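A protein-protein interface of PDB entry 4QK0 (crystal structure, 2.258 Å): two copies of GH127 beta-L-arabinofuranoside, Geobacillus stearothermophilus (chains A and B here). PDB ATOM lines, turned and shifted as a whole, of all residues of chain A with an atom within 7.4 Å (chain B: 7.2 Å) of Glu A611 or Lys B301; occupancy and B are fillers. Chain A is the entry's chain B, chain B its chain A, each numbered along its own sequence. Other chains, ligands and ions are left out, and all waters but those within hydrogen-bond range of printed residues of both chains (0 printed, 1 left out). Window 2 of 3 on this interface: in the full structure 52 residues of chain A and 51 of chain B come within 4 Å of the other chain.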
ATOM      1  N   GLU A 605       7.074  -1.422  -8.298  1.00  0.00           N
ATOM      2  CA  GLU A 605       6.993   0.068  -8.166  1.00  0.00           C
ATOM      3  C   GLU A 605       5.564   0.689  -8.255  1.00  0.00           C
ATOM      4  O   GLU A 605       5.247   1.710  -7.605  1.00  0.00           O
ATOM      5  CB  GLU A 605       7.806   0.697  -9.318  1.00  0.00           C
ATOM      6  CG  GLU A 605       8.552   1.969  -8.860  1.00  0.00           C
ATOM      7  CD  GLU A 605      10.049   1.936  -9.155  1.00  0.00           C
ATOM      8  OE1 GLU A 605      10.703   0.991  -8.656  1.00  0.00           O
ATOM      9  OE2 GLU A 605      10.574   2.873  -9.834  1.00  0.00           O
ATOM     10  N   SER A 606       4.709   0.037  -9.039  1.00  0.00           N
ATOM     11  CA  SER A 606       3.453   0.622  -9.484  1.00  0.00           C
ATOM     12  C   SER A 606       2.506   1.055  -8.406  1.00  0.00           C
ATOM     13  O   SER A 606       1.960   2.146  -8.467  1.00  0.00           O
ATOM     14  CB  SER A 606       2.734  -0.343 -10.387  1.00  0.00           C
ATOM     15  OG  SER A 606       3.552  -0.556 -11.520  1.00  0.00           O
ATOM     16  N   ALA A 607       2.282   0.213  -7.424  1.00  0.00           N
ATOM     17  CA  ALA A 607       1.271   0.515  -6.379  1.00  0.00           C
ATOM     18  C   ALA A 607       1.557   1.779  -5.533  1.00  0.00           C
ATOM     19  O   ALA A 607       0.717   2.220  -4.724  1.00  0.00           O
ATOM     20  CB  ALA A 607       1.122  -0.686  -5.457  1.00  0.00           C
ATOM     21  N   TRP A 608       2.757   2.340  -5.699  1.00  0.00           N
ATOM     22  CA  TRP A 608       3.089   3.608  -5.046  1.00  0.00           C
ATOM     23  C   TRP A 608       2.436   4.780  -5.808  1.00  0.00           C
ATOM     24  O   TRP A 608       1.837   5.630  -5.150  1.00  0.00           O
ATOM     25  CB  TRP A 608       4.632   3.787  -4.770  1.00  0.00           C
ATOM     26  CG  TRP A 608       4.974   3.190  -3.447  1.00  0.00           C
ATOM     27  CD1 TRP A 608       5.130   3.828  -2.246  1.00  0.00           C
ATOM     28  CD2 TRP A 608       5.061   1.791  -3.165  1.00  0.00           C
ATOM     29  NE1 TRP A 608       5.348   2.902  -1.249  1.00  0.00           N
ATOM     30  CE2 TRP A 608       5.301   1.649  -1.788  1.00  0.00           C
ATOM     31  CE3 TRP A 608       4.957   0.652  -3.946  1.00  0.00           C
ATOM     32  CZ2 TRP A 608       5.479   0.405  -1.186  1.00  0.00           C
ATOM     33  CZ3 TRP A 608       5.111  -0.615  -3.350  1.00  0.00           C
ATOM     34  CH2 TRP A 608       5.380  -0.736  -1.985  1.00  0.00           C
ATOM     35  N   ASN A 609       2.545   4.803  -7.149  1.00  0.00           N
ATOM     36  CA  ASN A 609       2.100   5.938  -7.987  1.00  0.00           C
ATOM     37  C   ASN A 609       2.701   7.264  -7.511  1.00  0.00           C
ATOM     38  O   ASN A 609       2.030   8.267  -7.214  1.00  0.00           O
ATOM     39  CB  ASN A 609       0.561   5.985  -8.239  1.00  0.00           C
ATOM     40  CG  ASN A 609      -0.258   6.274  -6.991  1.00  0.00           C
ATOM     41  OD1 ASN A 609       0.255   6.724  -5.959  1.00  0.00           O
ATOM     42  ND2 ASN A 609      -1.557   6.023  -7.082  1.00  0.00           N
ATOM     43  N   ASP A 610       4.014   7.230  -7.445  1.00  0.00           N
ATOM     44  CA  ASP A 610       4.772   8.394  -7.029  1.00  0.00           C
ATOM     45  C   ASP A 610       4.582   8.862  -5.588  1.00  0.00           C
ATOM     46  O   ASP A 610       5.099   9.893  -5.238  1.00  0.00           O
ATOM     47  CB  ASP A 610       4.460   9.571  -7.955  1.00  0.00           C
ATOM     48  CG  ASP A 610       4.632   9.218  -9.413  1.00  0.00           C
ATOM     49  OD1 ASP A 610       5.236   8.166  -9.709  1.00  0.00           O
ATOM     50  OD2 ASP A 610       4.169  10.000 -10.276  1.00  0.00           O
ATOM     51  N   GLU A 611       3.815   8.181  -4.766  1.00  0.00           N
ATOM     52  CA  GLU A 611       3.815   8.509  -3.348  1.00  0.00           C
ATOM     53  C   GLU A 611       5.154   7.998  -2.737  1.00  0.00           C
ATOM     54  O   GLU A 611       5.809   7.116  -3.299  1.00  0.00           O
ATOM     55  CB  GLU A 611       2.612   7.914  -2.636  1.00  0.00           C
ATOM     56  CG  GLU A 611       1.268   8.521  -3.037  1.00  0.00           C
ATOM     57  CD  GLU A 611       1.226  10.050  -2.843  1.00  0.00           C
ATOM     58  OE1 GLU A 611       0.940  10.769  -3.842  1.00  0.00           O
ATOM     59  OE2 GLU A 611       1.504  10.545  -1.711  1.00  0.00           O
ATOM     60  N   LEU A 612       5.573   8.595  -1.644  1.00  0.00           N
ATOM     61  CA  LEU A 612       6.787   8.190  -1.012  1.00  0.00           C
ATOM     62  C   LEU A 612       6.541   7.193   0.072  1.00  0.00           C
ATOM     63  O   LEU A 612       7.303   6.245   0.226  1.00  0.00           O
ATOM     64  CB  LEU A 612       7.564   9.410  -0.496  1.00  0.00           C
ATOM     65  CG  LEU A 612       8.934   9.230   0.103  1.00  0.00           C
ATOM     66  CD1 LEU A 612       9.869   8.506  -0.857  1.00  0.00           C
ATOM     67  CD2 LEU A 612       9.517  10.576   0.512  1.00  0.00           C
ATOM     68  N   TYR A 613       5.472   7.370   0.803  1.00  0.00           N
ATOM     69  CA  TYR A 613       5.073   6.486   1.888  1.00  0.00           C
ATOM     70  C   TYR A 613       3.619   6.073   1.717  1.00  0.00           C
ATOM     71  O   TYR A 613       2.818   6.906   1.408  1.00  0.00           O
ATOM     72  CB  TYR A 613       5.250   7.227   3.234  1.00  0.00           C
ATOM     73  CG  TYR A 613       6.661   7.698   3.439  1.00  0.00           C
ATOM     74  CD1 TYR A 613       7.707   6.774   3.483  1.00  0.00           C
ATOM     75  CD2 TYR A 613       6.987   9.046   3.522  1.00  0.00           C
ATOM     76  CE1 TYR A 613       8.977   7.179   3.647  1.00  0.00           C
ATOM     77  CE2 TYR A 613       8.297   9.460   3.680  1.00  0.00           C
ATOM     78  CZ  TYR A 613       9.291   8.520   3.715  1.00  0.00           C
ATOM     79  OH  TYR A 613      10.655   8.872   3.861  1.00  0.00           O
ATOM     80  N   ARG A 614       3.282   4.792   1.894  1.00  0.00           N
ATOM     81  CA  ARG A 614       1.927   4.266   1.661  1.00  0.00           C
ATOM     82  C   ARG A 614       1.612   3.169   2.652  1.00  0.00           C
ATOM     83  O   ARG A 614       2.446   2.288   2.870  1.00  0.00           O
ATOM     84  CB  ARG A 614       1.846   3.516   0.315  1.00  0.00           C
ATOM     85  CG  ARG A 614       1.598   4.172  -1.024  1.00  0.00           C
ATOM     86  CD  ARG A 614       0.306   4.945  -0.942  1.00  0.00           C
ATOM     87  NE  ARG A 614       0.522   6.282  -0.395  1.00  0.00           N
ATOM     88  CZ  ARG A 614      -0.447   7.154  -0.166  1.00  0.00           C
ATOM     89  NH1 ARG A 614      -1.712   6.836  -0.447  1.00  0.00           N
ATOM     90  NH2 ARG A 614      -0.146   8.351   0.323  1.00  0.00           N
ATOM     91  N   LEU B 295       9.406  22.063  -6.696  1.00  0.00           N
ATOM     92  CA  LEU B 295      10.279  21.849  -5.566  1.00  0.00           C
ATOM     93  C   LEU B 295       9.564  21.160  -4.425  1.00  0.00           C
ATOM     94  O   LEU B 295      10.134  20.286  -3.799  1.00  0.00           O
ATOM     95  CB  LEU B 295      10.901  23.144  -5.118  1.00  0.00           C
ATOM     96  CG  LEU B 295      11.942  23.651  -6.129  1.00  0.00           C
ATOM     97  CD1 LEU B 295      12.177  25.135  -5.976  1.00  0.00           C
ATOM     98  CD2 LEU B 295      13.262  22.938  -5.956  1.00  0.00           C
ATOM     99  N   TRP B 296       8.302  21.510  -4.197  1.00  0.00           N
ATOM    100  CA  TRP B 296       7.498  20.850  -3.207  1.00  0.00           C
ATOM    101  C   TRP B 296       7.402  19.371  -3.449  1.00  0.00           C
ATOM    102  O   TRP B 296       7.505  18.564  -2.524  1.00  0.00           O
ATOM    103  CB  TRP B 296       6.072  21.406  -3.208  1.00  0.00           C
ATOM    104  CG  TRP B 296       5.175  20.623  -2.345  1.00  0.00           C
ATOM    105  CD1 TRP B 296       4.324  19.663  -2.710  1.00  0.00           C
ATOM    106  CD2 TRP B 296       5.097  20.717  -0.936  1.00  0.00           C
ATOM    107  NE1 TRP B 296       3.700  19.145  -1.619  1.00  0.00           N
ATOM    108  CE2 TRP B 296       4.156  19.789  -0.515  1.00  0.00           C
ATOM    109  CE3 TRP B 296       5.707  21.538  -0.005  1.00  0.00           C
ATOM    110  CZ2 TRP B 296       3.798  19.643   0.781  1.00  0.00           C
ATOM    111  CZ3 TRP B 296       5.399  21.395   1.283  1.00  0.00           C
ATOM    112  CH2 TRP B 296       4.442  20.432   1.694  1.00  0.00           C
ATOM    113  N   GLU B 297       7.065  19.006  -4.658  1.00  0.00           N
ATOM    114  CA  GLU B 297       6.975  17.601  -5.018  1.00  0.00           C
ATOM    115  C   GLU B 297       8.328  16.905  -4.843  1.00  0.00           C
ATOM    116  O   GLU B 297       8.376  15.791  -4.363  1.00  0.00           O
ATOM    117  CB  GLU B 297       6.507  17.451  -6.473  1.00  0.00           C
ATOM    118  CG  GLU B 297       5.038  17.898  -6.651  1.00  0.00           C
ATOM    119  CD  GLU B 297       4.021  16.955  -5.988  1.00  0.00           C
ATOM    120  OE1 GLU B 297       3.959  15.769  -6.412  1.00  0.00           O
ATOM    121  OE2 GLU B 297       3.285  17.359  -5.039  1.00  0.00           O
ATOM    122  N   ASN B 298       9.426  17.561  -5.229  1.00  0.00           N
ATOM    123  CA  ASN B 298      10.700  16.934  -5.094  1.00  0.00           C
ATOM    124  C   ASN B 298      11.037  16.699  -3.599  1.00  0.00           C
ATOM    125  O   ASN B 298      11.479  15.611  -3.214  1.00  0.00           O
ATOM    126  CB  ASN B 298      11.780  17.745  -5.718  1.00  0.00           C
ATOM    127  CG  ASN B 298      13.131  17.011  -5.683  1.00  0.00           C
ATOM    128  OD1 ASN B 298      14.094  17.445  -5.047  1.00  0.00           O
ATOM    129  ND2 ASN B 298      13.214  15.919  -6.442  1.00  0.00           N
ATOM    130  N   VAL B 299      10.844  17.713  -2.761  1.00  0.00           N
ATOM    131  CA  VAL B 299      11.198  17.583  -1.341  1.00  0.00           C
ATOM    132  C   VAL B 299      10.319  16.515  -0.690  1.00  0.00           C
ATOM    133  O   VAL B 299      10.836  15.611  -0.055  1.00  0.00           O
ATOM    134  CB  VAL B 299      11.036  18.902  -0.577  1.00  0.00           C
ATOM    135  CG1 VAL B 299      11.137  18.658   0.895  1.00  0.00           C
ATOM    136  CG2 VAL B 299      12.089  19.861  -1.001  1.00  0.00           C
ATOM    137  N   THR B 300       9.012  16.595  -0.894  1.00  0.00           N
ATOM    138  CA  THR B 300       8.090  15.862  -0.074  1.00  0.00           C
ATOM    139  C   THR B 300       7.807  14.486  -0.640  1.00  0.00           C
ATOM    140  O   THR B 300       7.314  13.647   0.081  1.00  0.00           O
ATOM    141  CB  THR B 300       6.730  16.595   0.130  1.00  0.00           C
ATOM    142  OG1 THR B 300       6.051  16.743  -1.119  1.00  0.00           O
ATOM    143  CG2 THR B 300       6.954  17.908   0.735  1.00  0.00           C
ATOM    144  N   LYS B 301       8.051  14.273  -1.916  1.00  0.00           N
ATOM    145  CA  LYS B 301       7.883  12.956  -2.474  1.00  0.00           C
ATOM    146  C   LYS B 301       9.213  12.200  -2.751  1.00  0.00           C
ATOM    147  O   LYS B 301       9.190  11.055  -3.190  1.00  0.00           O
ATOM    148  CB  LYS B 301       7.069  13.032  -3.743  1.00  0.00           C
ATOM    149  CG  LYS B 301       5.647  13.474  -3.361  1.00  0.00           C
ATOM    150  CD  LYS B 301       4.460  12.926  -4.153  1.00  0.00           C
ATOM    151  CE  LYS B 301       3.148  13.499  -3.585  1.00  0.00           C
ATOM    152  NZ  LYS B 301       3.065  14.987  -3.772  1.00  0.00           N
ATOM    153  N   ARG B 302      10.346  12.865  -2.595  1.00  0.00           N
ATOM    154  CA  ARG B 302      11.618  12.194  -2.858  1.00  0.00           C
ATOM    155  C   ARG B 302      12.667  12.416  -1.837  1.00  0.00           C
ATOM    156  O   ARG B 302      13.560  11.618  -1.797  1.00  0.00           O
ATOM    157  CB  ARG B 302      12.136  12.565  -4.238  1.00  0.00           C
ATOM    158  CG  ARG B 302      11.115  12.221  -5.279  1.00  0.00           C
ATOM    159  CD  ARG B 302      11.675  12.230  -6.640  1.00  0.00           C
ATOM    160  NE  ARG B 302      10.755  11.625  -7.593  1.00  0.00           N
ATOM    161  CZ  ARG B 302      11.109  11.297  -8.833  1.00  0.00           C
ATOM    162  NH1 ARG B 302      12.363  11.484  -9.242  1.00  0.00           N
ATOM    163  NH2 ARG B 302      10.223  10.753  -9.654  1.00  0.00           N
ATOM    164  N   GLN B 303      12.604  13.488  -1.043  1.00  0.00           N
ATOM    165  CA  GLN B 303      13.709  13.802  -0.116  1.00  0.00           C
ATOM    166  C   GLN B 303      13.257  14.154   1.286  1.00  0.00           C
ATOM    167  O   GLN B 303      13.856  14.975   1.944  1.00  0.00           O
ATOM    168  CB  GLN B 303      14.609  14.877  -0.654  1.00  0.00           C
ATOM    169  CG  GLN B 303      15.255  14.500  -1.988  1.00  0.00           C
ATOM    170  CD  GLN B 303      16.385  15.456  -2.325  1.00  0.00           C
ATOM    171  OE1 GLN B 303      17.440  15.449  -1.695  1.00  0.00           O
ATOM    172  NE2 GLN B 303      16.128  16.373  -3.269  1.00  0.00           N
ATOM    173  N   MET B 304      12.225  13.484   1.755  1.00  0.00           N
ATOM    174  CA  MET B 304      11.691  13.720   3.054  1.00  0.00           C
ATOM    175  C   MET B 304      11.540  12.429   3.807  1.00  0.00           C
ATOM    176  O   MET B 304      11.055  11.461   3.261  1.00  0.00           O
ATOM    177  CB  MET B 304      10.295  14.359   2.937  1.00  0.00           C
ATOM    178  CG  MET B 304       9.731  14.717   4.269  1.00  0.00           C
ATOM    179  SD  MET B 304       7.863  15.423   4.191  1.00  0.00           S
ATOM    180  CE  MET B 304       6.928  13.838   3.680  1.00  0.00           C
ATOM    181  N   ASP B 322      17.348  12.339  -4.799  1.00  0.00           N
ATOM    182  CA  ASP B 322      16.121  11.549  -4.700  1.00  0.00           C
ATOM    183  C   ASP B 322      16.281  10.166  -4.085  1.00  0.00           C
ATOM    184  O   ASP B 322      17.114   9.371  -4.499  1.00  0.00           O
ATOM    185  CB  ASP B 322      15.514  11.392  -6.079  1.00  0.00           C
ATOM    186  CG  ASP B 322      15.059  12.749  -6.684  1.00  0.00           C
ATOM    187  OD1 ASP B 322      15.239  13.827  -6.046  1.00  0.00           O
ATOM    188  OD2 ASP B 322      14.551  12.715  -7.819  1.00  0.00           O
ATOM    189  N   PHE B 323      15.423   9.896  -3.114  1.00  0.00           N
ATOM    190  CA  PHE B 323      15.264   8.612  -2.511  1.00  0.00           C
ATOM    191  C   PHE B 323      16.444   8.162  -1.592  1.00  0.00           C
ATOM    192  O   PHE B 323      16.415   7.034  -1.126  1.00  0.00           O
ATOM    193  CB  PHE B 323      14.990   7.545  -3.558  1.00  0.00           C
ATOM    194  CG  PHE B 323      13.802   7.815  -4.439  1.00  0.00           C
ATOM    195  CD1 PHE B 323      12.515   7.859  -3.919  1.00  0.00           C
ATOM    196  CD2 PHE B 323      13.969   7.930  -5.815  1.00  0.00           C
ATOM    197  CE1 PHE B 323      11.422   8.016  -4.756  1.00  0.00           C
ATOM    198  CE2 PHE B 323      12.867   8.093  -6.666  1.00  0.00           C
ATOM    199  CZ  PHE B 323      11.596   8.160  -6.123  1.00  0.00           C
ATOM    200  N   LEU B 325      17.656   8.299   1.691  1.00  0.00           N
ATOM    201  CA  LEU B 325      17.088   8.617   3.003  1.00  0.00           C
ATOM    202  C   LEU B 325      17.502   7.616   4.076  1.00  0.00           C
ATOM    203  O   LEU B 325      16.670   6.878   4.625  1.00  0.00           O
ATOM    204  CB  LEU B 325      15.569   8.602   2.869  1.00  0.00           C
ATOM    205  CG  LEU B 325      15.051   9.750   2.004  1.00  0.00           C
ATOM    206  CD1 LEU B 325      13.614   9.483   1.636  1.00  0.00           C
ATOM    207  CD2 LEU B 325      15.174  11.104   2.700  1.00  0.00           C
ATOM    208  N   LYS B 355      -2.672  18.122   0.847  1.00  0.00           N
ATOM    209  CA  LYS B 355      -1.333  17.504   0.918  1.00  0.00           C
ATOM    210  C   LYS B 355      -0.311  18.401   1.583  1.00  0.00           C
ATOM    211  O   LYS B 355       0.604  17.915   2.199  1.00  0.00           O
ATOM    212  CB  LYS B 355      -0.858  17.033  -0.442  1.00  0.00           C
ATOM    213  CG  LYS B 355      -0.287  18.140  -1.334  1.00  0.00           C
ATOM    214  CD  LYS B 355      -0.246  17.749  -2.846  1.00  0.00           C
ATOM    215  CE  LYS B 355      -0.019  18.956  -3.746  1.00  0.00           C
ATOM    216  NZ  LYS B 355       0.880  18.737  -4.873  1.00  0.00           N
ATOM    217  N   LYS B 538       4.875   1.533   4.144  1.00  0.00           N
ATOM    218  CA  LYS B 538       5.959   1.151   3.280  1.00  0.00           C
ATOM    219  C   LYS B 538       6.518   2.320   2.495  1.00  0.00           C
ATOM    220  O   LYS B 538       5.773   3.197   2.071  1.00  0.00           O
ATOM    221  CB  LYS B 538       5.479   0.112   2.280  1.00  0.00           C
ATOM    222  CG  LYS B 538       5.030  -1.190   2.903  1.00  0.00           C
ATOM    223  CD  LYS B 538       6.140  -2.023   3.550  1.00  0.00           C
ATOM    224  CE  LYS B 538       7.292  -2.312   2.563  1.00  0.00           C
ATOM    225  NZ  LYS B 538       8.426  -3.087   3.111  1.00  0.00           N
ATOM    226  N   ALA B 539       7.832   2.346   2.317  1.00  0.00           N
ATOM    227  CA  ALA B 539       8.450   3.379   1.517  1.00  0.00           C
ATOM    228  C   ALA B 539       8.572   2.940   0.082  1.00  0.00           C
ATOM    229  O   ALA B 539       8.651   1.746  -0.221  1.00  0.00           O
ATOM    230  CB  ALA B 539       9.792   3.751   2.024  1.00  0.00           C
ATOM    231  N   HIS B 540       8.533   3.906  -0.823  1.00  0.00           N
ATOM    232  CA  HIS B 540       8.661   3.639  -2.247  1.00  0.00           C
ATOM    233  C   HIS B 540       9.900   2.718  -2.416  1.00  0.00           C
ATOM    234  O   HIS B 540      10.916   2.890  -1.700  1.00  0.00           O
ATOM    235  CB  HIS B 540       8.908   4.967  -2.934  1.00  0.00           C
ATOM    236  CG  HIS B 540       8.860   4.905  -4.400  1.00  0.00           C
ATOM    237  ND1 HIS B 540       9.824   4.273  -5.138  1.00  0.00           N
ATOM    238  CD2 HIS B 540       7.998   5.454  -5.287  1.00  0.00           C
ATOM    239  CE1 HIS B 540       9.559   4.417  -6.425  1.00  0.00           C
ATOM    240  NE2 HIS B 540       8.463   5.146  -6.541  1.00  0.00           N
ATOM    241  N   PRO B 541       9.847   1.765  -3.355  1.00  0.00           N
ATOM    242  CA  PRO B 541      10.949   0.792  -3.491  1.00  0.00           C
ATOM    243  C   PRO B 541      12.265   1.386  -3.865  1.00  0.00           C
ATOM    244  O   PRO B 541      13.249   0.760  -3.673  1.00  0.00           O
ATOM    245  CB  PRO B 541      10.455  -0.154  -4.569  1.00  0.00           C
ATOM    246  CG  PRO B 541       8.985  -0.091  -4.442  1.00  0.00           C
ATOM    247  CD  PRO B 541       8.657   1.335  -4.090  1.00  0.00           C
ATOM    248  N   VAL B 543      13.535   3.874  -2.324  1.00  0.00           N
ATOM    249  CA  VAL B 543      14.160   4.168  -1.032  1.00  0.00           C
ATOM    250  C   VAL B 543      14.866   2.946  -0.498  1.00  0.00           C
ATOM    251  O   VAL B 543      14.341   2.062   0.190  1.00  0.00           O
ATOM    252  CB  VAL B 543      13.188   4.683   0.003  1.00  0.00           C
ATOM    253  CG1 VAL B 543      13.976   5.088   1.253  1.00  0.00           C
ATOM    254  CG2 VAL B 543      12.453   5.907  -0.505  1.00  0.00           C
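O of Met B304 lies within hydrogen-bond range of OH of Tyr A613, at 2.7 Å. The backbone carbonyl oxygen (O) of Lys B538 is in hydrogen-bond range of the indole nitrogen (NE1) of Trp A608 (3.4 Å). O of Arg A614 lies within hydrogen-bond range of N of Lys B538, 2.8 Å away. N of His B540 is in hydrogen-bond range of O of Leu A612, at 2.8 Å. The indole nitrogen (NE1) of Trp A608 sits close to the backbone NH (N) of His B540 (3.4 Å).
The backbone carbonyl oxygen (O) of Trp B296 sits at hydrogen-bond distance from the side-chain hydroxyl (OG1) of Thr B300 (2.7 Å). NZ of Lys B301 is in salt-bridge range of OE2 of Glu B297 (2.7 Å). The backbone carbonyl oxygen (O) of Val B299 lies within hydrogen-bond range of the backbone NH (N) of Met B304 (3.1 Å). NH1 of Arg B302 is in salt-bridge range of OD2 of Asp B322 (2.9 Å). N of Phe B323 lies within hydrogen-bond range of O of Arg B302 (2.9 Å). The guanidinium group (NH2) of Arg A614 lies within salt-bridge range of the side-chain carboxylate (OE2) of Glu A611, at 3.4 Å.
Among the printed residues, pairs that only touch across the chains: Leu A612 with Met B304, Asp A610 with Lys B301, Leu A612 with Ala B539, Tyr A613 with Lys B538, Glu A611 with His B540, Trp A608 with Ala B539, Glu A611 with Lys B301, Leu A612 with Lys B301, Glu A605 with His B540, Leu A612 with Val B543, Trp A608 with Pro B541, Tyr A613 with Leu B325, Leu A612 with Thr B300, Leu A612 with Lys B538, Tyr A613 with Ala B539 and Leu A612 with Arg B302.
Asn A609 touches none of the printed residues of chain B. Glu A611 touches just these residues of chain B: Lys B301 (3.5 Å) and His B540 (3.4 Å). Of the printed residues of chain B, Leu A612 touches Thr B300 (3.8 Å), Lys B301 (3.5 Å), Arg B302 (3.9 Å), Met B304 (3.3 Å), Lys B538 (3.9 Å), Ala B539 (3.3 Å), His B540 (2.8 Å) and Val B543 (3.7 Å). Of the printed residues of chain B, Arg A614 touches Lys B538 (2.8 Å). Glu B297 touches none of the printed residues of chain A. Printed residues of chain A within 4 Å of Thr B300: Leu A612 (3.8 Å). Lys B301 touches just these residues of chain A: Asp A610, Glu A611 and Leu A612. Of the printed residues of chain A, Leu B325 touches Tyr A613 (3.8 Å).
Of the 19 printed residues of chain B, 10 touch a printed residue of chain A. Hydrophobic or aromatic side chains of chain B that line the printed part of chain A: Leu B325, Ala B539, His B540, Pro B541 and Val B543. Among the printed residues, 21 pairs touch across the chains.
No position is printed for both chains.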
